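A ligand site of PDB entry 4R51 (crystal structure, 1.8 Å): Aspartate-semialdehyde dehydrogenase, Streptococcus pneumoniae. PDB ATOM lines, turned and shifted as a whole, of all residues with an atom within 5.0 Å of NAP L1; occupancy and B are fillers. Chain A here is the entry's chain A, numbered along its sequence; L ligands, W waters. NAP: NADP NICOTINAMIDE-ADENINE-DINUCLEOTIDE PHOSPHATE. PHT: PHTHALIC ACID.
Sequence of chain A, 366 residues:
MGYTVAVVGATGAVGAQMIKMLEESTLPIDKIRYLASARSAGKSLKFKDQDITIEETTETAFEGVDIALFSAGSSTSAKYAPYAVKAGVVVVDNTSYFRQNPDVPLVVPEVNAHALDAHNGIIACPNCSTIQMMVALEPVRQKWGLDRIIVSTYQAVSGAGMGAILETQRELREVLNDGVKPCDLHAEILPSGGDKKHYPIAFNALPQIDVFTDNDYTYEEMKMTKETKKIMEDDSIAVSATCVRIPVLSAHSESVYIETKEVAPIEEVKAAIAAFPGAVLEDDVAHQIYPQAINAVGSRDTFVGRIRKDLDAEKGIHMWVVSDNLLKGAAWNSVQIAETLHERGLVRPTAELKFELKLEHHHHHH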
ATOM      1  N   GLY A   9       8.682  -9.624   4.654  1.00  0.00           N
ATOM      2  CA  GLY A   9       8.468 -10.085   6.009  1.00  0.00           C
ATOM      3  C   GLY A   9       6.982 -10.175   6.331  1.00  0.00           C
ATOM      4  O   GLY A   9       6.550  -9.797   7.412  1.00  0.00           O
ATOM      5  N   ALA A  10       6.203 -10.701   5.393  1.00  0.00           N
ATOM      6  CA  ALA A  10       4.742 -10.757   5.531  1.00  0.00           C
ATOM      7  C   ALA A  10       4.246 -11.710   6.628  1.00  0.00           C
ATOM      8  O   ALA A  10       3.120 -11.558   7.108  1.00  0.00           O
ATOM      9  CB  ALA A  10       4.116 -11.119   4.194  1.00  0.00           C
ATOM     10  N   THR A  11       5.070 -12.687   7.012  1.00  0.00           N
ATOM     11  CA  THR A  11       4.698 -13.732   7.960  1.00  0.00           C
ATOM     12  C   THR A  11       4.934 -13.409   9.436  1.00  0.00           C
ATOM     13  O   THR A  11       4.556 -14.207  10.300  1.00  0.00           O
ATOM     14  CB  THR A  11       5.498 -15.024   7.663  1.00  0.00           C
ATOM     15  OG1 THR A  11       6.885 -14.697   7.567  1.00  0.00           O
ATOM     16  CG2 THR A  11       5.049 -15.638   6.370  1.00  0.00           C
ATOM     17  N   GLY A  12       5.552 -12.274   9.731  1.00  0.00           N
ATOM     18  CA  GLY A  12       5.894 -11.937  11.116  1.00  0.00           C
ATOM     19  C   GLY A  12       4.861 -11.071  11.827  1.00  0.00           C
ATOM     20  O   GLY A  12       3.759 -10.856  11.298  1.00  0.00           O
ATOM     21  N   ALA A  13       5.225 -10.600  13.017  1.00  0.00           N
ATOM     22  CA  ALA A  13       4.380  -9.766  13.862  1.00  0.00           C
ATOM     23  C   ALA A  13       4.020  -8.464  13.171  1.00  0.00           C
ATOM     24  O   ALA A  13       2.849  -8.108  13.102  1.00  0.00           O
ATOM     25  CB  ALA A  13       5.070  -9.474  15.197  1.00  0.00           C
ATOM     26  N   VAL A  14       5.030  -7.760  12.637  1.00  0.00           N
ATOM     27  CA  VAL A  14       4.768  -6.507  11.932  1.00  0.00           C
ATOM     28  C   VAL A  14       4.072  -6.784  10.609  1.00  0.00           C
ATOM     29  O   VAL A  14       3.114  -6.090  10.264  1.00  0.00           O
ATOM     30  CB  VAL A  14       6.049  -5.685  11.679  1.00  0.00           C
ATOM     31  CG1 VAL A  14       5.767  -4.528  10.719  1.00  0.00           C
ATOM     32  CG2 VAL A  14       6.630  -5.178  12.995  1.00  0.00           C
ATOM     33  N   GLY A  15       4.566  -7.779   9.874  1.00  0.00           N
ATOM     34  CA  GLY A  15       3.934  -8.241   8.630  1.00  0.00           C
ATOM     35  C   GLY A  15       2.432  -8.498   8.723  1.00  0.00           C
ATOM     36  O   GLY A  15       1.683  -8.097   7.818  1.00  0.00           O
ATOM     37  N   ALA A  36       9.005 -13.382   2.122  1.00  0.00           N
ATOM     38  CA  ALA A  36       9.601 -13.740   3.396  1.00  0.00           C
ATOM     39  C   ALA A  36      10.835 -14.607   3.121  1.00  0.00           C
ATOM     40  O   ALA A  36      11.510 -14.389   2.116  1.00  0.00           O
ATOM     41  CB  ALA A  36       8.589 -14.443   4.278  1.00  0.00           C
ATOM     42  N   SER A  37      11.172 -15.526   4.017  1.00  0.00           N
ATOM     43  CA  SER A  37      12.352 -16.374   3.829  1.00  0.00           C
ATOM     44  C   SER A  37      12.013 -17.529   2.905  1.00  0.00           C
ATOM     45  O   SER A  37      10.845 -17.809   2.663  1.00  0.00           O
ATOM     46  CB  SER A  37      12.822 -16.947   5.175  1.00  0.00           C
ATOM     47  OG  SER A  37      11.974 -18.004   5.574  1.00  0.00           O
ATOM     48  N   ARG A  39      12.044 -20.518   3.674  1.00  0.00           N
ATOM     49  CA  ARG A  39      11.215 -21.435   4.471  1.00  0.00           C
ATOM     50  C   ARG A  39       9.737 -21.186   4.245  1.00  0.00           C
ATOM     51  O   ARG A  39       8.951 -22.113   4.101  1.00  0.00           O
ATOM     52  CB  ARG A  39      11.513 -21.305   5.969  1.00  0.00           C
ATOM     53  CG  ARG A  39      12.928 -21.690   6.375  1.00  0.00           C
ATOM     54  CD  ARG A  39      13.170 -21.412   7.861  1.00  0.00           C
ATOM     55  NE  ARG A  39      12.985 -20.000   8.207  1.00  0.00           N
ATOM     56  CZ  ARG A  39      13.901 -19.041   8.080  1.00  0.00           C
ATOM     57  NH1 ARG A  39      15.124 -19.306   7.618  1.00  0.00           N
ATOM     58  NH2 ARG A  39      13.605 -17.793   8.423  1.00  0.00           N
ATOM     59  N   SER A  40       9.347 -19.909   4.227  1.00  0.00           N
ATOM     60  CA  SER A  40       7.951 -19.547   4.009  1.00  0.00           C
ATOM     61  C   SER A  40       7.526 -19.611   2.541  1.00  0.00           C
ATOM     62  O   SER A  40       6.347 -19.778   2.251  1.00  0.00           O
ATOM     63  CB  SER A  40       7.666 -18.145   4.577  1.00  0.00           C
ATOM     64  OG  SER A  40       7.645 -18.205   5.985  1.00  0.00           O
ATOM     65  N   THR A  57      12.482 -13.784  -0.583  1.00  0.00           N
ATOM     66  CA  THR A  57      13.057 -12.448  -0.799  1.00  0.00           C
ATOM     67  C   THR A  57      14.404 -12.597  -1.509  1.00  0.00           C
ATOM     68  O   THR A  57      15.323 -13.215  -0.975  1.00  0.00           O
ATOM     69  CB  THR A  57      13.216 -11.693   0.530  1.00  0.00           C
ATOM     70  OG1 THR A  57      11.965 -11.696   1.223  1.00  0.00           O
ATOM     71  CG2 THR A  57      13.661 -10.258   0.286  1.00  0.00           C
ATOM     72  N   SER A  71       9.753  -5.191   6.413  1.00  0.00           N
ATOM     73  CA  SER A  71       9.836  -5.409   7.849  1.00  0.00           C
ATOM     74  C   SER A  71      10.316  -6.826   8.167  1.00  0.00           C
ATOM     75  O   SER A  71       9.639  -7.583   8.871  1.00  0.00           O
ATOM     76  CB  SER A  71       8.478  -5.114   8.501  1.00  0.00           C
ATOM     77  OG  SER A  71       8.682  -4.947   9.896  1.00  0.00           O
ATOM     78  N   ALA A  72      11.486  -7.179   7.610  1.00  0.00           N
ATOM     79  CA  ALA A  72      12.048  -8.521   7.767  1.00  0.00           C
ATOM     80  C   ALA A  72      13.448  -8.513   8.418  1.00  0.00           C
ATOM     81  O   ALA A  72      14.203  -9.490   8.288  1.00  0.00           O
ATOM     82  CB  ALA A  72      12.122  -9.198   6.402  1.00  0.00           C
ATOM     83  N   GLY A  73      13.788  -7.424   9.092  1.00  0.00           N
ATOM     84  CA  GLY A  73      15.053  -7.332   9.815  1.00  0.00           C
ATOM     85  C   GLY A  73      16.048  -6.440   9.103  1.00  0.00           C
ATOM     86  O   GLY A  73      16.020  -6.338   7.872  1.00  0.00           O
ATOM     87  N   SER A  74      16.919  -5.785   9.864  1.00  0.00           N
ATOM     88  CA  SER A  74      17.835  -4.815   9.304  1.00  0.00           C
ATOM     89  C   SER A  74      18.747  -5.430   8.256  1.00  0.00           C
ATOM     90  O   SER A  74      19.038  -4.800   7.236  1.00  0.00           O
ATOM     91  CB  SER A  74      18.676  -4.152  10.411  1.00  0.00           C
ATOM     92  OG  SER A  74      17.842  -3.361  11.250  1.00  0.00           O
ATOM     93  N   THR A  76      18.101  -7.968   6.243  1.00  0.00           N
ATOM     94  CA  THR A  76      17.313  -8.157   5.020  1.00  0.00           C
ATOM     95  C   THR A  76      17.139  -6.848   4.246  1.00  0.00           C
ATOM     96  O   THR A  76      17.261  -6.808   3.023  1.00  0.00           O
ATOM     97  CB  THR A  76      15.954  -8.808   5.341  1.00  0.00           C
ATOM     98  OG1 THR A  76      16.180 -10.043   6.042  1.00  0.00           O
ATOM     99  CG2 THR A  76      15.153  -9.093   4.086  1.00  0.00           C
ATOM    100  N   LYS A  79      20.534  -5.835   2.645  1.00  0.00           N
ATOM    101  CA  LYS A  79      20.835  -6.686   1.495  1.00  0.00           C
ATOM    102  C   LYS A  79      19.945  -6.431   0.283  1.00  0.00           C
ATOM    103  O   LYS A  79      20.445  -6.432  -0.833  1.00  0.00           O
ATOM    104  CB  LYS A  79      20.713  -8.148   1.891  1.00  0.00           C
ATOM    105  CG  LYS A  79      21.845  -8.679   2.769  1.00  0.00           C
ATOM    106  CD  LYS A  79      21.643 -10.162   3.074  1.00  0.00           C
ATOM    107  CE  LYS A  79      20.594 -10.383   4.146  1.00  0.00           C
ATOM    108  NZ  LYS A  79      20.025 -11.762   4.134  1.00  0.00           N
ATOM    109  N   ASN A  94      10.935  -0.391   7.515  1.00  0.00           N
ATOM    110  CA  ASN A  94      10.632  -0.357   8.970  1.00  0.00           C
ATOM    111  C   ASN A  94      11.841  -0.561   9.898  1.00  0.00           C
ATOM    112  O   ASN A  94      11.756  -0.325  11.102  1.00  0.00           O
ATOM    113  CB  ASN A  94       9.544  -1.393   9.343  1.00  0.00           C
ATOM    114  CG  ASN A  94       8.148  -0.805   9.371  1.00  0.00           C
ATOM    115  OD1 ASN A  94       7.265  -1.262   8.636  1.00  0.00           O
ATOM    116  ND2 ASN A  94       7.937   0.207  10.218  1.00  0.00           N
ATOM    117  N   THR A  95      12.987  -0.939   9.331  1.00  0.00           N
ATOM    118  CA  THR A  95      14.141  -1.304  10.140  1.00  0.00           C
ATOM    119  C   THR A  95      15.019  -0.080  10.428  1.00  0.00           C
ATOM    120  O   THR A  95      14.816   0.992   9.861  1.00  0.00           O
ATOM    121  CB  THR A  95      15.019  -2.384   9.454  1.00  0.00           C
ATOM    122  OG1 THR A  95      15.898  -1.757   8.513  1.00  0.00           O
ATOM    123  CG2 THR A  95      14.147  -3.429   8.755  1.00  0.00           C
ATOM    124  N   SER A  96      16.011  -0.280  11.294  1.00  0.00           N
ATOM    125  CA  SER A  96      16.940   0.769  11.676  1.00  0.00           C
ATOM    126  C   SER A  96      18.029   1.045  10.635  1.00  0.00           C
ATOM    127  O   SER A  96      18.723   2.058  10.731  1.00  0.00           O
ATOM    128  CB  SER A  96      17.614   0.434  13.003  1.00  0.00           C
ATOM    129  OG  SER A  96      18.399  -0.751  12.883  1.00  0.00           O
ATOM    130  N   ARG A  99      18.068   4.518   8.622  1.00  0.00           N
ATOM    131  CA  ARG A  99      17.423   5.675   9.272  1.00  0.00           C
ATOM    132  C   ARG A  99      18.322   6.907   9.391  1.00  0.00           C
ATOM    133  O   ARG A  99      17.826   8.035   9.268  1.00  0.00           O
ATOM    134  CB  ARG A  99      16.936   5.306  10.664  1.00  0.00           C
ATOM    135  CG  ARG A  99      15.770   4.350  10.669  1.00  0.00           C
ATOM    136  CD  ARG A  99      15.230   4.202  12.075  1.00  0.00           C
ATOM    137  NE  ARG A  99      14.139   3.237  12.105  1.00  0.00           N
ATOM    138  CZ  ARG A  99      13.959   2.313  13.044  1.00  0.00           C
ATOM    139  NH1 ARG A  99      14.775   2.228  14.093  1.00  0.00           N
ATOM    140  NH2 ARG A  99      12.950   1.467  12.922  1.00  0.00           N
ATOM    141  N   CYS A 125      10.925   4.318   8.139  1.00  0.00           N
ATOM    142  CA  CYS A 125      10.002   4.436   9.249  1.00  0.00           C
ATOM    143  C   CYS A 125      10.854   4.428  10.531  1.00  0.00           C
ATOM    144  O   CYS A 125      11.753   3.584  10.658  1.00  0.00           O
ATOM    145  CB  CYS A 125       8.995   3.272   9.215  1.00  0.00           C
ATOM    146  SG  CYS A 125       7.758   3.208  10.544  1.00  0.00           S
ATOM    147  N   PRO A 126      10.610   5.379  11.459  1.00  0.00           N
ATOM    148  CA  PRO A 126      11.393   5.381  12.701  1.00  0.00           C
ATOM    149  C   PRO A 126      11.042   4.239  13.647  1.00  0.00           C
ATOM    150  O   PRO A 126      10.105   3.475  13.417  1.00  0.00           O
ATOM    151  CB  PRO A 126      11.069   6.735  13.349  1.00  0.00           C
ATOM    152  CG  PRO A 126      10.336   7.526  12.318  1.00  0.00           C
ATOM    153  CD  PRO A 126       9.717   6.545  11.375  1.00  0.00           C
ATOM    154  N   ASN A 127      11.825   4.118  14.712  1.00  0.00           N
ATOM    155  CA  ASN A 127      11.545   3.135  15.753  1.00  0.00           C
ATOM    156  C   ASN A 127      10.202   3.459  16.425  1.00  0.00           C
ATOM    157  O   ASN A 127       9.867   4.620  16.611  1.00  0.00           O
ATOM    158  CB  ASN A 127      12.668   3.132  16.773  1.00  0.00           C
ATOM    159  CG  ASN A 127      12.419   2.146  17.897  1.00  0.00           C
ATOM    160  OD1 ASN A 127      12.575   0.933  17.737  1.00  0.00           O
ATOM    161  ND2 ASN A 127      12.021   2.662  19.033  1.00  0.00           N
ATOM    162  N   CYS A 128       9.464   2.411  16.806  1.00  0.00           N
ATOM    163  CA  CYS A 128       8.115   2.569  17.388  1.00  0.00           C
ATOM    164  C   CYS A 128       8.083   3.536  18.567  1.00  0.00           C
ATOM    165  O   CYS A 128       7.219   4.419  18.639  1.00  0.00           O
ATOM    166  CB  CYS A 128       7.564   1.216  17.818  1.00  0.00           C
ATOM    167  SG  CYS A 128       8.733   0.264  18.781  1.00  0.00           S
ATOM    168  N   ILE A 131       8.350   7.108  17.309  1.00  0.00           N
ATOM    169  CA  ILE A 131       7.216   7.610  16.550  1.00  0.00           C
ATOM    170  C   ILE A 131       6.157   8.218  17.480  1.00  0.00           C
ATOM    171  O   ILE A 131       5.733   9.342  17.240  1.00  0.00           O
ATOM    172  CB  ILE A 131       6.575   6.543  15.640  1.00  0.00           C
ATOM    173  CG1 ILE A 131       7.554   6.122  14.522  1.00  0.00           C
ATOM    174  CG2 ILE A 131       5.312   7.089  15.007  1.00  0.00           C
ATOM    175  CD1 ILE A 131       7.169   4.817  13.838  1.00  0.00           C
ATOM    176  N   SER A 158       5.550  -7.450  21.919  1.00  0.00           N
ATOM    177  CA  SER A 158       5.267  -7.645  20.494  1.00  0.00           C
ATOM    178  C   SER A 158       6.292  -6.942  19.616  1.00  0.00           C
ATOM    179  O   SER A 158       6.507  -7.340  18.472  1.00  0.00           O
ATOM    180  CB  SER A 158       3.858  -7.220  20.106  1.00  0.00           C
ATOM    181  OG  SER A 158       3.686  -5.821  20.222  1.00  0.00           O
ATOM    182  N   GLY A 159       6.925  -5.892  20.160  1.00  0.00           N
ATOM    183  CA  GLY A 159       7.996  -5.194  19.475  1.00  0.00           C
ATOM    184  C   GLY A 159       9.220  -6.052  19.185  1.00  0.00           C
ATOM    185  O   GLY A 159      10.012  -5.707  18.318  1.00  0.00           O
ATOM    186  N   ALA A 160       9.370  -7.163  19.914  1.00  0.00           N
ATOM    187  CA  ALA A 160      10.483  -8.078  19.734  1.00  0.00           C
ATOM    188  C   ALA A 160      10.147  -9.293  18.854  1.00  0.00           C
ATOM    189  O   ALA A 160      10.988 -10.184  18.700  1.00  0.00           O
ATOM    190  CB  ALA A 160      11.005  -8.533  21.084  1.00  0.00           C
ATOM    191  N   GLY A 161       8.948  -9.338  18.299  1.00  0.00           N
ATOM    192  CA  GLY A 161       8.581 -10.342  17.305  1.00  0.00           C
ATOM    193  C   GLY A 161       7.695 -11.451  17.820  1.00  0.00           C
ATOM    194  O   GLY A 161       7.420 -11.574  19.020  1.00  0.00           O
ATOM    195  N   MET A 162       7.245 -12.281  16.887  1.00  0.00           N
ATOM    196  CA  MET A 162       6.330 -13.369  17.180  1.00  0.00           C
ATOM    197  C   MET A 162       6.884 -14.304  18.253  1.00  0.00           C
ATOM    198  O   MET A 162       6.153 -14.716  19.147  1.00  0.00           O
ATOM    199  CB  MET A 162       6.030 -14.165  15.897  1.00  0.00           C
ATOM    200  CG  MET A 162       4.585 -14.540  15.712  1.00  0.00           C
ATOM    201  SD  MET A 162       3.467 -13.115  15.740  1.00  0.00           S
ATOM    202  CE  MET A 162       2.533 -13.382  14.239  1.00  0.00           C
ATOM    203  N   ASN A 325       2.242  -0.302  19.370  1.00  0.00           N
ATOM    204  CA  ASN A 325       3.596  -0.320  18.796  1.00  0.00           C
ATOM    205  C   ASN A 325       3.691  -0.992  17.433  1.00  0.00           C
ATOM    206  O   ASN A 325       4.667  -0.773  16.703  1.00  0.00           O
ATOM    207  CB  ASN A 325       4.572  -0.980  19.775  1.00  0.00           C
ATOM    208  CG  ASN A 325       4.193  -2.407  20.086  1.00  0.00           C
ATOM    209  OD1 ASN A 325       3.175  -2.641  20.702  1.00  0.00           O
ATOM    210  ND2 ASN A 325       4.972  -3.363  19.604  1.00  0.00           N
ATOM    211  N   LEU A 326       2.704  -1.835  17.099  1.00  0.00           N
ATOM    212  CA  LEU A 326       2.661  -2.471  15.783  1.00  0.00           C
ATOM    213  C   LEU A 326       1.861  -1.688  14.754  1.00  0.00           C
ATOM    214  O   LEU A 326       1.974  -1.963  13.561  1.00  0.00           O
ATOM    215  CB  LEU A 326       2.119  -3.895  15.873  1.00  0.00           C
ATOM    216  CG  LEU A 326       2.935  -4.889  16.693  1.00  0.00           C
ATOM    217  CD1 LEU A 326       2.346  -6.289  16.549  1.00  0.00           C
ATOM    218  CD2 LEU A 326       4.395  -4.885  16.287  1.00  0.00           C
ATOM    219  N   GLY A 329       3.360   2.631  15.663  1.00  0.00           N
ATOM    220  CA  GLY A 329       4.753   2.318  15.885  1.00  0.00           C
ATOM    221  C   GLY A 329       5.456   1.586  14.767  1.00  0.00           C
ATOM    222  O   GLY A 329       6.687   1.463  14.779  1.00  0.00           O
ATOM    223  N   ALA A 330       4.704   1.055  13.794  1.00  0.00           N
ATOM    224  CA  ALA A 330       5.314   0.277  12.713  1.00  0.00           C
ATOM    225  C   ALA A 330       4.437   0.195  11.451  1.00  0.00           C
ATOM    226  O   ALA A 330       4.634   0.979  10.529  1.00  0.00           O
ATOM    227  CB  ALA A 330       5.694  -1.114  13.208  1.00  0.00           C
HETATM  228  PA  NAP L   1       9.080 -11.546  13.539  1.00  0.00           P
HETATM  229  O1A NAP L   1      10.196 -12.381  14.097  1.00  0.00           O
HETATM  230  O2A NAP L   1       7.690 -11.625  14.122  1.00  0.00           O
HETATM  231  O5B NAP L   1       9.057 -11.781  11.955  1.00  0.00           O
HETATM  232  C5B NAP L   1      10.263 -11.856  11.209  1.00  0.00           C
HETATM  233  C4B NAP L   1       9.935 -11.715   9.738  1.00  0.00           C
HETATM  234  O4B NAP L   1      11.161 -11.589   9.011  1.00  0.00           O
HETATM  235  C3B NAP L   1       9.223 -12.937   9.163  1.00  0.00           C
HETATM  236  O3B NAP L   1       8.320 -12.559   8.123  1.00  0.00           O
HETATM  237  C2B NAP L   1      10.361 -13.734   8.593  1.00  0.00           C
HETATM  238  O2B NAP L   1       9.988 -14.677   7.584  1.00  0.00           O
HETATM  239  C1B NAP L   1      11.205 -12.609   8.022  1.00  0.00           C
HETATM  240  N9A NAP L   1      12.555 -13.103   7.704  1.00  0.00           N
HETATM  241  C8A NAP L   1      13.411 -13.733   8.527  1.00  0.00           C
HETATM  242  N7A NAP L   1      14.529 -14.082   7.862  1.00  0.00           N
HETATM  243  C5A NAP L   1      14.395 -13.682   6.590  1.00  0.00           C
HETATM  244  C6A NAP L   1      15.196 -13.734   5.347  1.00  0.00           C
HETATM  245  N6A NAP L   1      16.419 -14.303   5.340  1.00  0.00           N
HETATM  246  N1A NAP L   1      14.674 -13.208   4.224  1.00  0.00           N
HETATM  247  C2A NAP L   1      13.456 -12.637   4.214  1.00  0.00           C
HETATM  248  N3A NAP L   1      12.677 -12.548   5.303  1.00  0.00           N
HETATM  249  C4A NAP L   1      13.079 -13.042   6.486  1.00  0.00           C
HETATM  250  O3  NAP L   1       9.628 -10.020  13.675  1.00  0.00           O
HETATM  251  PN  NAP L   1       8.788  -8.645  13.579  1.00  0.00           P
HETATM  252  O1N NAP L   1       8.342  -8.197  14.949  1.00  0.00           O
HETATM  253  O2N NAP L   1       7.751  -8.738  12.499  1.00  0.00           O
HETATM  254  O5D NAP L   1       9.921  -7.622  13.141  1.00  0.00           O
HETATM  255  C5D NAP L   1      10.723  -7.848  11.986  1.00  0.00           C
HETATM  256  C4D NAP L   1      11.567  -6.601  11.763  1.00  0.00           C
HETATM  257  O4D NAP L   1      10.745  -5.428  11.581  1.00  0.00           O
HETATM  258  C3D NAP L   1      12.470  -6.287  12.939  1.00  0.00           C
HETATM  259  O3D NAP L   1      13.683  -7.049  12.924  1.00  0.00           O
HETATM  260  C2D NAP L   1      12.694  -4.806  12.763  1.00  0.00           C
HETATM  261  O2D NAP L   1      13.771  -4.581  11.848  1.00  0.00           O
HETATM  262  C1D NAP L   1      11.376  -4.297  12.187  1.00  0.00           C
HETATM  263  N1N NAP L   1      10.555  -3.722  13.257  1.00  0.00           N
HETATM  264  C2N NAP L   1      10.511  -2.380  13.400  1.00  0.00           C
HETATM  265  C3N NAP L   1       9.748  -1.793  14.411  1.00  0.00           C
HETATM  266  C7N NAP L   1       9.717  -0.313  14.583  1.00  0.00           C
HETATM  267  O7N NAP L   1       9.921   0.121  15.702  1.00  0.00           O
HETATM  268  N7N NAP L   1       9.496   0.492  13.545  1.00  0.00           N
HETATM  269  C4N NAP L   1       9.027  -2.597  15.292  1.00  0.00           C
HETATM  270  C5N NAP L   1       9.086  -3.973  15.132  1.00  0.00           C
HETATM  271  C6N NAP L   1       9.860  -4.505  14.106  1.00  0.00           C
HETATM  272  P2B NAP L   1       9.850 -16.273   7.876  1.00  0.00           P
HETATM  273  O1X NAP L   1       8.508 -16.404   8.544  1.00  0.00           O
HETATM  274  O2X NAP L   1       9.934 -16.884   6.514  1.00  0.00           O
HETATM  275  O3X NAP L   1      11.040 -16.570   8.764  1.00  0.00           O
HETATM  276  O8  PHT L   2      14.827  -0.268  15.312  1.00  0.00           O
HETATM  277  O9  PHT L   2      12.755  -0.570  14.741  1.00  0.00           O
HETATM  278  C10 PHT L   2      15.995  -2.818  14.030  1.00  0.00           C
HETATM  279  O11 PHT L   2      17.171  -2.585  14.386  1.00  0.00           O
HETATM  280  O12 PHT L   2      15.609  -2.623  12.868  1.00  0.00           O
HETATM  281  C7  PHT L   2      13.833  -1.006  15.175  1.00  0.00           C
HETATM  282  C1  PHT L   2      15.006  -4.686  15.390  1.00  0.00           C
HETATM  283  C2  PHT L   2      14.986  -3.346  15.009  1.00  0.00           C
HETATM  284  C3  PHT L   2      13.921  -2.464  15.551  1.00  0.00           C
HETATM  285  C4  PHT L   2      12.993  -3.004  16.428  1.00  0.00           C
HETATM  286  C5  PHT L   2      13.071  -4.351  16.792  1.00  0.00           C
HETATM  287  C6  PHT L   2      14.064  -5.175  16.279  1.00  0.00           C
HETATM  288  O   HOH W   1      16.529  -6.388  12.634  1.00  0.00           O
HETATM  289  O   HOH W   2       7.792 -16.362  11.445  1.00  0.00           O
HETATM  290  O   HOH W   3      10.780  -7.120  16.187  1.00  0.00           O
HETATM  291  O   HOH W   4       7.044  -9.204  10.091  1.00  0.00           O
HETATM  292  O   HOH W   5      10.188 -14.112  16.106  1.00  0.00           O
HETATM  293  O   HOH W   6      15.433 -14.597   1.657  1.00  0.00           O
HETATM  294  O   HOH W   7      12.985  -8.629  15.476  1.00  0.00           O
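An oxygen (O3B) of NAP L1 lies within hydrogen-bond range of the backbone NH (N) of Thr 11 (3.4 Å).
O2N of NAP L1 is in hydrogen-bond range of N of Val 14, at 2.9 Å.
O11 of PHT L2 sits at hydrogen-bond distance from OG of Ser 96, 2.7 Å away.
The backbone carbonyl oxygen of Pro 126 is in hydrogen-bond range of a nitrogen (N7N) of NAP L1, at 3.0 Å.
An oxygen (O1X) of NAP L1 lies within hydrogen-bond range of the side-chain hydroxyl (OG1) of Thr 11 (2.6 Å).
The backbone NH (N) of Met 162 sits at hydrogen-bond distance from an oxygen (O2A) of NAP L1, at 2.9 Å.
O2X of NAP L1 is in hydrogen-bond range of OG of Ser 40 (2.7 Å).
The guanidinium group (NH2) of Arg 39 lies within salt-bridge range of an oxygen (O3X) of NAP L1, 2.9 Å away.
An oxygen (O2A) of NAP L1 is in hydrogen-bond range of the backbone NH (N) of Ala 13, at 2.9 Å.
The side-chain hydroxyl (OG) of Ser 71 sits at hydrogen-bond distance from an oxygen (O4D) of NAP L1 (2.7 Å).
The side-chain hydroxyl (OG) of Ser 37 sits at hydrogen-bond distance from an oxygen (O2X) of NAP L1 (2.5 Å).
The backbone NH (N) of Ser 96 sits at hydrogen-bond distance from an oxygen (O12) of PHT L2 (2.9 Å).
N of Ser 37 is in hydrogen-bond range of O2X of NAP L1, at 3.1 Å.
A nitrogen (N7N) of NAP L1 lies close to the backbone carbonyl oxygen of Asn 94 (3.4 Å).
An oxygen (O9) of PHT L2 sits close to the side-chain amide oxygen (OD1) of Asn 127.
The backbone NH (N) of Gly 12 is in hydrogen-bond range of an oxygen (O3B) of NAP L1, 3.2 Å away.
OD1 of Asn 127 sits close to O7N of NAP L1 (3.4 Å).
A nitrogen (N7N) of NAP L1 is in hydrogen-bond range of the backbone carbonyl oxygen (O) of Gly 329, 3.2 Å away.
O9 of PHT L2 is in salt-bridge range of NH2 of Arg 99 (2.7 Å).
The side-chain hydroxyl of Ser 74 sits at hydrogen-bond distance from an oxygen (O12) of PHT L2.
An oxygen (O7N) of NAP L1 lies within hydrogen-bond range of the side-chain sulfur of Cys 128 (3.3 Å).
An oxygen (O7N) of NAP L1 sits at hydrogen-bond distance from the backbone NH (N) of Cys 128 (2.6 Å).
The backbone carbonyl oxygen of Gly 9 lies close to an oxygen (O3B) of NAP L1 (3.4 Å).
O2D of NAP L1 lies within hydrogen-bond range of O12 of PHT L2.
The side-chain hydroxyl (OG1) of Thr 76 lies within hydrogen-bond range of the backbone carbonyl oxygen (O) of Ala 72, 3.0 Å away.
The backbone carbonyl oxygen of Cys 125 is in hydrogen-bond range of the guanidinium group of Arg 99, at 2.8 Å.
O of Ala 36 sits at hydrogen-bond distance from OG1 of Thr 57 (2.9 Å).
The backbone NH (N) of Gly 159 lies close to the side-chain amide nitrogen (ND2) of Asn 325 (3.2 Å).
OG of Ser 74 sits at hydrogen-bond distance from OG of Ser 96, 3.1 Å away.
The side-chain amide nitrogen (ND2) of Asn 94 is in hydrogen-bond range of the backbone carbonyl oxygen (O) of Ala 330 (3.4 Å).
The side-chain hydroxyl (OG) of Ser 37 lies close to the backbone NH (N) of Arg 39, 3.2 Å away.
O of Thr 95 is in hydrogen-bond range of NE of Arg 99, 3.2 Å away.
Residues that only touch NAP L1: Ala 10 (3.9 Å), Ala 36 (3.4 Å), Thr 57 (3.5 Å), Ala 72 (3.4 Å), Gly 73 (3.4 Å), Ser 74 (3.9 Å), Thr 76 (3.9 Å), Thr 95 (3.3 Å), Arg 99 (3.6 Å), Gly 159 (3.7 Å) and Gly 161 (3.2 Å).
Hydrophobic or aromatic side chains that line NAP L1: Ala 13, Val 14, Ala 36, Ala 72 and Met 162.
26 residues have an atom within 4 Å of NAP L1: Gly 9, Ala 10, Thr 11, Gly 12, Ala 13, Val 14, Ala 36, Ser 37, Arg 39, Ser 40, Thr 57, Ser 71, Ala 72, Gly 73, Ser 74, Thr 76, Asn 94, Thr 95, Arg 99, Pro 126, Asn 127, Cys 128, Gly 159, Gly 161, Met 162 and Gly 329.
Water W4 lies within hydrogen-bond range of O2N of NAP L1, O of Gly 9, N of Gly 15, O of Ser 71 and N of Gly 12.
Water W1 lies within hydrogen-bond range of the backbone NH of Ser 74 and an oxygen (O3D) of NAP L1.
Water W3 bridges O of Gly 159 and O1N of NAP L1.
Water W6 lies within hydrogen-bond range of the backbone carbonyl oxygen (O) of Thr 57 and a nitrogen (N1A) of NAP L1.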
